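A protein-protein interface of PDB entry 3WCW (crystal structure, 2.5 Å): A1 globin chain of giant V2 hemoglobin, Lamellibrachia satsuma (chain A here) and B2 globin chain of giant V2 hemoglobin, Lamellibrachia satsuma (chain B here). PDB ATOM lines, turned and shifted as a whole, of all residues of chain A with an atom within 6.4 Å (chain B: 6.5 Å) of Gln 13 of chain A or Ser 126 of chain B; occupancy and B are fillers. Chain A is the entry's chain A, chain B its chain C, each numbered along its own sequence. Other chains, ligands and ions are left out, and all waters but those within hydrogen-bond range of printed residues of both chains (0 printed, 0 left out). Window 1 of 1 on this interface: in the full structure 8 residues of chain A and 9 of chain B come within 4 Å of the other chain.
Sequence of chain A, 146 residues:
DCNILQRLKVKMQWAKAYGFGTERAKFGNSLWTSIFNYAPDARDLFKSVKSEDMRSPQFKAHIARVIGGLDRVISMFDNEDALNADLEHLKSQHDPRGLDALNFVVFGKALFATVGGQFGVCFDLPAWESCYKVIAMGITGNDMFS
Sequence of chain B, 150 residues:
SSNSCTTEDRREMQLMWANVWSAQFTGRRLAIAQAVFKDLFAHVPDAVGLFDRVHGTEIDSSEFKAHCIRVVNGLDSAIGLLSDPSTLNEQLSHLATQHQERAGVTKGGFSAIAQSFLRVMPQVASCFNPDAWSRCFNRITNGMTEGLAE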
ATOM      1  N   LEU A   8       1.440  -3.898 -22.688  1.00  0.00           N
ATOM      2  CA  LEU A   8       1.449  -4.470 -21.351  1.00  0.00           C
ATOM      3  C   LEU A   8       0.742  -5.830 -21.361  1.00  0.00           C
ATOM      4  O   LEU A   8       1.214  -6.795 -20.760  1.00  0.00           O
ATOM      5  CB  LEU A   8       0.745  -3.529 -20.372  1.00  0.00           C
ATOM      6  CG  LEU A   8       1.488  -2.233 -20.034  1.00  0.00           C
ATOM      7  CD1 LEU A   8       0.748  -1.489 -18.922  1.00  0.00           C
ATOM      8  CD2 LEU A   8       2.918  -2.560 -19.594  1.00  0.00           C
ATOM      9  N   LYS A   9      -0.397  -5.891 -22.042  1.00  0.00           N
ATOM     10  CA  LYS A   9      -1.161  -7.124 -22.138  1.00  0.00           C
ATOM     11  C   LYS A   9      -0.264  -8.186 -22.784  1.00  0.00           C
ATOM     12  O   LYS A   9      -0.161  -9.318 -22.300  1.00  0.00           O
ATOM     13  CB  LYS A   9      -2.415  -6.889 -22.989  1.00  0.00           C
ATOM     14  CG  LYS A   9      -3.228  -8.143 -23.279  1.00  0.00           C
ATOM     15  CD  LYS A   9      -4.008  -8.637 -22.066  1.00  0.00           C
ATOM     16  CE  LYS A   9      -5.315  -7.874 -21.894  1.00  0.00           C
ATOM     17  NZ  LYS A   9      -6.390  -8.287 -22.853  1.00  0.00           N
ATOM     18  N   VAL A  10       0.394  -7.795 -23.872  1.00  0.00           N
ATOM     19  CA  VAL A  10       1.292  -8.681 -24.605  1.00  0.00           C
ATOM     20  C   VAL A  10       2.490  -9.153 -23.755  1.00  0.00           C
ATOM     21  O   VAL A  10       2.847 -10.341 -23.794  1.00  0.00           O
ATOM     22  CB  VAL A  10       1.783  -7.976 -25.912  1.00  0.00           C
ATOM     23  CG1 VAL A  10       3.023  -8.647 -26.457  1.00  0.00           C
ATOM     24  CG2 VAL A  10       0.673  -8.018 -26.961  1.00  0.00           C
ATOM     25  N   LYS A  11       3.108  -8.241 -22.994  1.00  0.00           N
ATOM     26  CA  LYS A  11       4.245  -8.612 -22.147  1.00  0.00           C
ATOM     27  C   LYS A  11       3.818  -9.676 -21.142  1.00  0.00           C
ATOM     28  O   LYS A  11       4.533 -10.646 -20.912  1.00  0.00           O
ATOM     29  CB  LYS A  11       4.805  -7.384 -21.402  1.00  0.00           C
ATOM     30  CG  LYS A  11       5.784  -6.554 -22.226  1.00  0.00           C
ATOM     31  CD  LYS A  11       5.950  -5.122 -21.694  1.00  0.00           C
ATOM     32  CE  LYS A  11       6.854  -5.042 -20.467  1.00  0.00           C
ATOM     33  NZ  LYS A  11       8.283  -5.337 -20.770  1.00  0.00           N
ATOM     34  N   MET A  12       2.641  -9.481 -20.561  1.00  0.00           N
ATOM     35  CA  MET A  12       2.087 -10.398 -19.582  1.00  0.00           C
ATOM     36  C   MET A  12       1.745 -11.762 -20.212  1.00  0.00           C
ATOM     37  O   MET A  12       2.207 -12.799 -19.740  1.00  0.00           O
ATOM     38  CB  MET A  12       0.827  -9.794 -18.965  1.00  0.00           C
ATOM     39  CG  MET A  12       0.610 -10.134 -17.504  1.00  0.00           C
ATOM     40  SD  MET A  12       1.108  -8.752 -16.414  1.00  0.00           S
ATOM     41  CE  MET A  12       2.864  -9.209 -16.026  1.00  0.00           C
ATOM     42  N   GLN A  13       0.939 -11.774 -21.270  1.00  0.00           N
ATOM     43  CA  GLN A  13       0.576 -13.046 -21.889  1.00  0.00           C
ATOM     44  C   GLN A  13       1.820 -13.809 -22.381  1.00  0.00           C
ATOM     45  O   GLN A  13       1.893 -15.034 -22.265  1.00  0.00           O
ATOM     46  CB  GLN A  13      -0.410 -12.825 -23.040  1.00  0.00           C
ATOM     47  CG  GLN A  13      -1.656 -12.025 -22.652  1.00  0.00           C
ATOM     48  CD  GLN A  13      -2.873 -12.373 -23.496  1.00  0.00           C
ATOM     49  OE1 GLN A  13      -2.749 -12.806 -24.650  1.00  0.00           O
ATOM     50  NE2 GLN A  13      -4.064 -12.178 -22.928  1.00  0.00           N
ATOM     51  N   TRP A  14       2.802 -13.075 -22.904  1.00  0.00           N
ATOM     52  CA  TRP A  14       4.034 -13.684 -23.391  1.00  0.00           C
ATOM     53  C   TRP A  14       4.818 -14.357 -22.259  1.00  0.00           C
ATOM     54  O   TRP A  14       5.296 -15.488 -22.406  1.00  0.00           O
ATOM     55  CB  TRP A  14       4.912 -12.627 -24.080  1.00  0.00           C
ATOM     56  CG  TRP A  14       6.360 -13.019 -24.194  1.00  0.00           C
ATOM     57  CD1 TRP A  14       7.387 -12.642 -23.365  1.00  0.00           C
ATOM     58  CD2 TRP A  14       6.927 -13.929 -25.141  1.00  0.00           C
ATOM     59  NE1 TRP A  14       8.557 -13.268 -23.737  1.00  0.00           N
ATOM     60  CE2 TRP A  14       8.305 -14.059 -24.824  1.00  0.00           C
ATOM     61  CE3 TRP A  14       6.407 -14.650 -26.223  1.00  0.00           C
ATOM     62  CZ2 TRP A  14       9.158 -14.870 -25.549  1.00  0.00           C
ATOM     63  CZ3 TRP A  14       7.254 -15.454 -26.943  1.00  0.00           C
ATOM     64  CH2 TRP A  14       8.620 -15.560 -26.606  1.00  0.00           C
ATOM     65  N   ALA A  15       4.958 -13.658 -21.140  1.00  0.00           N
ATOM     66  CA  ALA A  15       5.696 -14.187 -19.995  1.00  0.00           C
ATOM     67  C   ALA A  15       5.107 -15.516 -19.529  1.00  0.00           C
ATOM     68  O   ALA A  15       5.822 -16.476 -19.275  1.00  0.00           O
ATOM     69  CB  ALA A  15       5.686 -13.168 -18.847  1.00  0.00           C
ATOM     70  N   LYS A  16       3.793 -15.566 -19.434  1.00  0.00           N
ATOM     71  CA  LYS A  16       3.119 -16.771 -18.997  1.00  0.00           C
ATOM     72  C   LYS A  16       3.330 -17.952 -19.958  1.00  0.00           C
ATOM     73  O   LYS A  16       3.641 -19.056 -19.527  1.00  0.00           O
ATOM     74  CB  LYS A  16       1.621 -16.473 -18.833  1.00  0.00           C
ATOM     75  CG  LYS A  16       0.787 -17.625 -18.289  1.00  0.00           C
ATOM     76  CD  LYS A  16       1.171 -17.989 -16.848  1.00  0.00           C
ATOM     77  CE  LYS A  16       0.323 -19.163 -16.324  1.00  0.00           C
ATOM     78  NZ  LYS A  16       0.641 -19.529 -14.904  1.00  0.00           N
ATOM     79  N   ALA A  17       3.169 -17.709 -21.258  1.00  0.00           N
ATOM     80  CA  ALA A  17       3.294 -18.758 -22.279  1.00  0.00           C
ATOM     81  C   ALA A  17       4.710 -19.249 -22.548  1.00  0.00           C
ATOM     82  O   ALA A  17       4.928 -20.429 -22.836  1.00  0.00           O
ATOM     83  CB  ALA A  17       2.661 -18.276 -23.582  1.00  0.00           C
ATOM     84  N   TYR A  18       5.661 -18.325 -22.478  1.00  0.00           N
ATOM     85  CA  TYR A  18       7.079 -18.603 -22.704  1.00  0.00           C
ATOM     86  C   TYR A  18       7.655 -19.455 -21.568  1.00  0.00           C
ATOM     87  O   TYR A  18       8.484 -20.333 -21.795  1.00  0.00           O
ATOM     88  CB  TYR A  18       7.827 -17.277 -22.799  1.00  0.00           C
ATOM     89  CG  TYR A  18       9.298 -17.382 -23.082  1.00  0.00           C
ATOM     90  CD1 TYR A  18       9.770 -18.076 -24.198  1.00  0.00           C
ATOM     91  CD2 TYR A  18      10.217 -16.698 -22.290  1.00  0.00           C
ATOM     92  CE1 TYR A  18      11.133 -18.070 -24.529  1.00  0.00           C
ATOM     93  CE2 TYR A  18      11.571 -16.684 -22.608  1.00  0.00           C
ATOM     94  CZ  TYR A  18      12.023 -17.365 -23.732  1.00  0.00           C
ATOM     95  OH  TYR A  18      13.359 -17.292 -24.069  1.00  0.00           O
ATOM     96  N   VAL A 115       1.234 -18.970 -28.725  1.00  0.00           N
ATOM     97  CA  VAL A 115       1.052 -18.281 -27.447  1.00  0.00           C
ATOM     98  C   VAL A 115      -0.346 -18.539 -26.900  1.00  0.00           C
ATOM     99  O   VAL A 115      -0.520 -18.839 -25.709  1.00  0.00           O
ATOM    100  CB  VAL A 115       1.248 -16.753 -27.578  1.00  0.00           C
ATOM    101  CG1 VAL A 115       0.950 -16.064 -26.233  1.00  0.00           C
ATOM    102  CG2 VAL A 115       2.667 -16.448 -28.040  1.00  0.00           C
ATOM    103  N   PHE A 119      -1.312 -20.140 -23.636  1.00  0.00           N
ATOM    104  CA  PHE A 119      -1.894 -19.211 -22.671  1.00  0.00           C
ATOM    105  C   PHE A 119      -3.348 -19.485 -22.275  1.00  0.00           C
ATOM    106  O   PHE A 119      -3.762 -19.194 -21.149  1.00  0.00           O
ATOM    107  CB  PHE A 119      -1.793 -17.785 -23.207  1.00  0.00           C
ATOM    108  CG  PHE A 119      -2.167 -16.743 -22.203  1.00  0.00           C
ATOM    109  CD1 PHE A 119      -1.274 -16.383 -21.195  1.00  0.00           C
ATOM    110  CD2 PHE A 119      -3.429 -16.159 -22.228  1.00  0.00           C
ATOM    111  CE1 PHE A 119      -1.637 -15.458 -20.226  1.00  0.00           C
ATOM    112  CE2 PHE A 119      -3.809 -15.232 -21.266  1.00  0.00           C
ATOM    113  CZ  PHE A 119      -2.915 -14.878 -20.261  1.00  0.00           C
ATOM    114  N   CYS A 122      -8.021 -16.807 -22.650  1.00  0.00           N
ATOM    115  CA  CYS A 122      -7.980 -15.364 -22.450  1.00  0.00           C
ATOM    116  C   CYS A 122      -6.953 -14.667 -23.335  1.00  0.00           C
ATOM    117  O   CYS A 122      -6.712 -13.471 -23.211  1.00  0.00           O
ATOM    118  CB  CYS A 122      -7.788 -15.032 -20.956  1.00  0.00           C
ATOM    119  SG  CYS A 122      -9.108 -15.812 -19.942  1.00  0.00           S
ATOM    120  N   PHE A 123      -6.366 -15.427 -24.250  1.00  0.00           N
ATOM    121  CA  PHE A 123      -5.404 -14.894 -25.206  1.00  0.00           C
ATOM    122  C   PHE A 123      -6.091 -13.718 -25.923  1.00  0.00           C
ATOM    123  O   PHE A 123      -7.233 -13.838 -26.366  1.00  0.00           O
ATOM    124  CB  PHE A 123      -5.040 -15.997 -26.215  1.00  0.00           C
ATOM    125  CG  PHE A 123      -4.168 -15.536 -27.353  1.00  0.00           C
ATOM    126  CD1 PHE A 123      -2.892 -15.001 -27.107  1.00  0.00           C
ATOM    127  CD2 PHE A 123      -4.600 -15.680 -28.672  1.00  0.00           C
ATOM    128  CE1 PHE A 123      -2.058 -14.619 -28.163  1.00  0.00           C
ATOM    129  CE2 PHE A 123      -3.782 -15.304 -29.734  1.00  0.00           C
ATOM    130  CZ  PHE A 123      -2.502 -14.771 -29.478  1.00  0.00           C
ATOM    131  N   ASP A 124      -5.404 -12.582 -26.018  1.00  0.00           N
ATOM    132  CA  ASP A 124      -5.959 -11.397 -26.667  1.00  0.00           C
ATOM    133  C   ASP A 124      -5.445 -11.360 -28.101  1.00  0.00           C
ATOM    134  O   ASP A 124      -4.471 -10.667 -28.392  1.00  0.00           O
ATOM    135  CB  ASP A 124      -5.497 -10.141 -25.921  1.00  0.00           C
ATOM    136  CG  ASP A 124      -6.210  -8.875 -26.383  1.00  0.00           C
ATOM    137  OD1 ASP A 124      -6.463  -8.719 -27.606  1.00  0.00           O
ATOM    138  OD2 ASP A 124      -6.496  -8.025 -25.515  1.00  0.00           O
ATOM    139  N   LEU A 125      -6.089 -12.102 -29.002  1.00  0.00           N
ATOM    140  CA  LEU A 125      -5.642 -12.130 -30.394  1.00  0.00           C
ATOM    141  C   LEU A 125      -5.465 -10.729 -31.035  1.00  0.00           C
ATOM    142  O   LEU A 125      -4.447 -10.467 -31.676  1.00  0.00           O
ATOM    143  CB  LEU A 125      -6.577 -13.001 -31.247  1.00  0.00           C
ATOM    144  CG  LEU A 125      -6.161 -13.058 -32.726  1.00  0.00           C
ATOM    145  CD1 LEU A 125      -4.714 -13.548 -32.851  1.00  0.00           C
ATOM    146  CD2 LEU A 125      -7.095 -13.959 -33.489  1.00  0.00           C
ATOM    147  N   TRP A 128      -2.281  -8.958 -29.945  1.00  0.00           N
ATOM    148  CA  TRP A 128      -1.106  -9.603 -30.501  1.00  0.00           C
ATOM    149  C   TRP A 128      -0.948  -9.304 -31.987  1.00  0.00           C
ATOM    150  O   TRP A 128       0.169  -9.153 -32.466  1.00  0.00           O
ATOM    151  CB  TRP A 128      -1.137 -11.113 -30.249  1.00  0.00           C
ATOM    152  CG  TRP A 128      -0.677 -11.500 -28.858  1.00  0.00           C
ATOM    153  CD1 TRP A 128      -1.425 -11.505 -27.708  1.00  0.00           C
ATOM    154  CD2 TRP A 128       0.646 -11.902 -28.472  1.00  0.00           C
ATOM    155  NE1 TRP A 128      -0.651 -11.882 -26.642  1.00  0.00           N
ATOM    156  CE2 TRP A 128       0.623 -12.130 -27.081  1.00  0.00           C
ATOM    157  CE3 TRP A 128       1.849 -12.090 -29.170  1.00  0.00           C
ATOM    158  CZ2 TRP A 128       1.754 -12.535 -26.371  1.00  0.00           C
ATOM    159  CZ3 TRP A 128       2.974 -12.495 -28.468  1.00  0.00           C
ATOM    160  CH2 TRP A 128       2.918 -12.713 -27.075  1.00  0.00           C
ATOM    161  N   LEU B  15      -8.163 -11.195  -8.407  1.00  0.00           N
ATOM    162  CA  LEU B  15      -7.456 -11.926  -9.446  1.00  0.00           C
ATOM    163  C   LEU B  15      -7.273 -11.026 -10.671  1.00  0.00           C
ATOM    164  O   LEU B  15      -6.189 -10.961 -11.244  1.00  0.00           O
ATOM    165  CB  LEU B  15      -8.224 -13.184  -9.861  1.00  0.00           C
ATOM    166  CG  LEU B  15      -8.051 -14.470  -9.051  1.00  0.00           C
ATOM    167  CD1 LEU B  15      -8.875 -15.569  -9.728  1.00  0.00           C
ATOM    168  CD2 LEU B  15      -6.575 -14.884  -8.973  1.00  0.00           C
ATOM    169  N   MET B  16      -8.341 -10.347 -11.081  1.00  0.00           N
ATOM    170  CA  MET B  16      -8.264  -9.455 -12.228  1.00  0.00           C
ATOM    171  C   MET B  16      -7.225  -8.389 -11.946  1.00  0.00           C
ATOM    172  O   MET B  16      -6.472  -8.007 -12.829  1.00  0.00           O
ATOM    173  CB  MET B  16      -9.612  -8.770 -12.493  1.00  0.00           C
ATOM    174  CG  MET B  16     -10.695  -9.671 -13.040  1.00  0.00           C
ATOM    175  SD  MET B  16     -12.223  -8.755 -13.357  1.00  0.00           S
ATOM    176  CE  MET B  16     -13.213  -9.266 -11.976  1.00  0.00           C
ATOM    177  N   ASN B  19      -3.328 -10.074 -11.695  1.00  0.00           N
ATOM    178  CA  ASN B  19      -2.821 -10.405 -13.021  1.00  0.00           C
ATOM    179  C   ASN B  19      -2.788  -9.177 -13.923  1.00  0.00           C
ATOM    180  O   ASN B  19      -3.061  -9.264 -15.128  1.00  0.00           O
ATOM    181  CB  ASN B  19      -3.678 -11.507 -13.655  1.00  0.00           C
ATOM    182  CG  ASN B  19      -3.552 -12.838 -12.924  1.00  0.00           C
ATOM    183  OD1 ASN B  19      -3.877 -12.947 -11.737  1.00  0.00           O
ATOM    184  ND2 ASN B  19      -3.073 -13.856 -13.631  1.00  0.00           N
ATOM    185  N   VAL B  20      -2.450  -8.036 -13.326  1.00  0.00           N
ATOM    186  CA  VAL B  20      -2.356  -6.774 -14.042  1.00  0.00           C
ATOM    187  C   VAL B  20      -1.499  -5.798 -13.245  1.00  0.00           C
ATOM    188  O   VAL B  20      -0.981  -4.828 -13.789  1.00  0.00           O
ATOM    189  CB  VAL B  20      -3.737  -6.141 -14.234  1.00  0.00           C
ATOM    190  CG1 VAL B  20      -3.620  -4.863 -15.036  1.00  0.00           C
ATOM    191  CG2 VAL B  20      -4.658  -7.114 -14.928  1.00  0.00           C
ATOM    192  N   MET B 121      -9.597  -1.659 -18.257  1.00  0.00           N
ATOM    193  CA  MET B 121      -9.305  -3.014 -17.813  1.00  0.00           C
ATOM    194  C   MET B 121      -9.245  -4.133 -18.873  1.00  0.00           C
ATOM    195  O   MET B 121      -8.257  -4.864 -18.953  1.00  0.00           O
ATOM    196  CB  MET B 121     -10.285  -3.410 -16.713  1.00  0.00           C
ATOM    197  CG  MET B 121     -10.095  -2.628 -15.426  1.00  0.00           C
ATOM    198  SD  MET B 121      -8.426  -2.776 -14.750  1.00  0.00           S
ATOM    199  CE  MET B 121      -8.484  -4.451 -14.086  1.00  0.00           C
ATOM    200  N   PRO B 122     -10.292  -4.287 -19.691  1.00  0.00           N
ATOM    201  CA  PRO B 122     -10.248  -5.351 -20.701  1.00  0.00           C
ATOM    202  C   PRO B 122      -9.035  -5.318 -21.637  1.00  0.00           C
ATOM    203  O   PRO B 122      -8.615  -6.345 -22.161  1.00  0.00           O
ATOM    204  CB  PRO B 122     -11.568  -5.176 -21.448  1.00  0.00           C
ATOM    205  CG  PRO B 122     -11.875  -3.724 -21.285  1.00  0.00           C
ATOM    206  CD  PRO B 122     -11.498  -3.458 -19.848  1.00  0.00           C
ATOM    207  N   VAL B 124      -5.964  -4.358 -20.735  1.00  0.00           N
ATOM    208  CA  VAL B 124      -4.771  -4.745 -20.004  1.00  0.00           C
ATOM    209  C   VAL B 124      -4.855  -6.070 -19.227  1.00  0.00           C
ATOM    210  O   VAL B 124      -3.863  -6.794 -19.115  1.00  0.00           O
ATOM    211  CB  VAL B 124      -4.371  -3.604 -19.042  1.00  0.00           C
ATOM    212  CG1 VAL B 124      -5.348  -3.528 -17.881  1.00  0.00           C
ATOM    213  CG2 VAL B 124      -2.955  -3.802 -18.568  1.00  0.00           C
ATOM    214  N   ALA B 125      -6.031  -6.384 -18.698  1.00  0.00           N
ATOM    215  CA  ALA B 125      -6.228  -7.608 -17.926  1.00  0.00           C
ATOM    216  C   ALA B 125      -6.726  -8.761 -18.778  1.00  0.00           C
ATOM    217  O   ALA B 125      -7.502  -8.567 -19.714  1.00  0.00           O
ATOM    218  CB  ALA B 125      -7.209  -7.359 -16.801  1.00  0.00           C
ATOM    219  N   SER B 126      -6.289  -9.966 -18.432  1.00  0.00           N
ATOM    220  CA  SER B 126      -6.686 -11.167 -19.153  1.00  0.00           C
ATOM    221  C   SER B 126      -7.845 -11.819 -18.407  1.00  0.00           C
ATOM    222  O   SER B 126      -7.827 -11.878 -17.179  1.00  0.00           O
ATOM    223  CB  SER B 126      -5.515 -12.158 -19.229  1.00  0.00           C
ATOM    224  OG  SER B 126      -4.404 -11.617 -19.929  1.00  0.00           O
ATOM    225  N   CYS B 127      -8.851 -12.297 -19.139  1.00  0.00           N
ATOM    226  CA  CYS B 127      -9.993 -12.964 -18.507  1.00  0.00           C
ATOM    227  C   CYS B 127     -10.868 -11.988 -17.733  1.00  0.00           C
ATOM    228  O   CYS B 127     -11.604 -12.406 -16.834  1.00  0.00           O
ATOM    229  CB  CYS B 127      -9.531 -14.012 -17.489  1.00  0.00           C
ATOM    230  SG  CYS B 127      -8.552 -15.451 -18.025  1.00  0.00           S
ATOM    231  N   PHE B 128     -10.778 -10.702 -18.059  1.00  0.00           N
ATOM    232  CA  PHE B 128     -11.550  -9.680 -17.363  1.00  0.00           C
ATOM    233  C   PHE B 128     -13.032  -9.972 -17.301  1.00  0.00           C
ATOM    234  O   PHE B 128     -13.649 -10.307 -18.315  1.00  0.00           O
ATOM    235  CB  PHE B 128     -11.359  -8.321 -18.024  1.00  0.00           C
ATOM    236  CG  PHE B 128     -12.069  -7.200 -17.313  1.00  0.00           C
ATOM    237  CD1 PHE B 128     -11.646  -6.779 -16.050  1.00  0.00           C
ATOM    238  CD2 PHE B 128     -13.145  -6.545 -17.915  1.00  0.00           C
ATOM    239  CE1 PHE B 128     -12.281  -5.719 -15.395  1.00  0.00           C
ATOM    240  CE2 PHE B 128     -13.791  -5.484 -17.272  1.00  0.00           C
ATOM    241  CZ  PHE B 128     -13.357  -5.072 -16.010  1.00  0.00           C
ATOM    242  N   ASN B 129     -13.594  -9.844 -16.102  1.00  0.00           N
ATOM    243  CA  ASN B 129     -15.020 -10.049 -15.889  1.00  0.00           C
ATOM    244  C   ASN B 129     -15.615  -8.716 -15.430  1.00  0.00           C
ATOM    245  O   ASN B 129     -15.533  -8.366 -14.251  1.00  0.00           O
ATOM    246  CB  ASN B 129     -15.270 -11.121 -14.829  1.00  0.00           C
ATOM    247  CG  ASN B 129     -16.752 -11.397 -14.633  1.00  0.00           C
ATOM    248  OD1 ASN B 129     -17.596 -10.787 -15.294  1.00  0.00           O
ATOM    249  ND2 ASN B 129     -17.077 -12.317 -13.729  1.00  0.00           N
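Of the printed residues of chain B, Lys 9 of chain A touches Pro 122 (3.0 Å), Val 124 (3.3 Å), Ala 125 (3.2 Å) and Ser 126 (3.7 Å). Gln 13 of chain A touches one residue of chain B. Phe 123 of chain A touches none of the printed residues of chain B. Printed residues of chain A within 4 Å of Pro 122 of chain B: Lys 9 (3.0 Å). Of chain A, only Lys 9, Gln 13 and Phe 119 come within 4 Å of Ser 126 of chain B. The nearest residue of chain A that does not touch Ser 126 of chain B is Cys 122 of chain A (4.1 Å). The nearest printed residue of chain A that does not touch Cys 127 of chain B is Phe 119 of chain A (5.7 Å).
Printed residues of chain B that touch a printed residue of chain A: Pro 122, Val 124, Ala 125, Ser 126 and Cys 127. Among the printed residues, no Asp or Glu carboxylate lies within 4 Å of a Lys or Arg side-chain nitrogen of the other chain.
OE1 of Gln 13 of chain A is in hydrogen-bond range of NE1 of Trp 128 of chain A (3.0 Å). NZ of Lys 9 of chain A lies within salt-bridge range of OD2 of Asp 124 of chain A, 2.7 Å away. NE2 of Gln 13 of chain A lies within hydrogen-bond range of O of Cys 122 of chain A (3.0 Å). N of Asp 124 of chain A lies within hydrogen-bond range of OE1 of Gln 13 of chain A (3.0 Å).
CE of Lys 9 of chain A touches C of Val 124 of chain B, 3.3 Å away. OG of Ser 126 of chain B touches CD of Lys 9 of chain A (3.7 Å). Phe 119 of chain A touches Ser 126 of chain B (CZ to OG, 3.6 Å).
SG of Cys 122 of chain A is disulfide-bonded to SG of Cys 127 of chain B (2.0 Å). OG of Ser 126 of chain B is in hydrogen-bond range of NE2 of Gln 13 of chain A (3.1 Å). The side-chain amino group (NZ) of Lys 9 of chain A sits close to the backbone carbonyl oxygen (O) of Ala 125 of chain B, at 3.3 Å. The side-chain amino group (NZ) of Lys 9 of chain A lies within hydrogen-bond range of the backbone carbonyl oxygen (O) of Pro 122 of chain B (3.0 Å).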
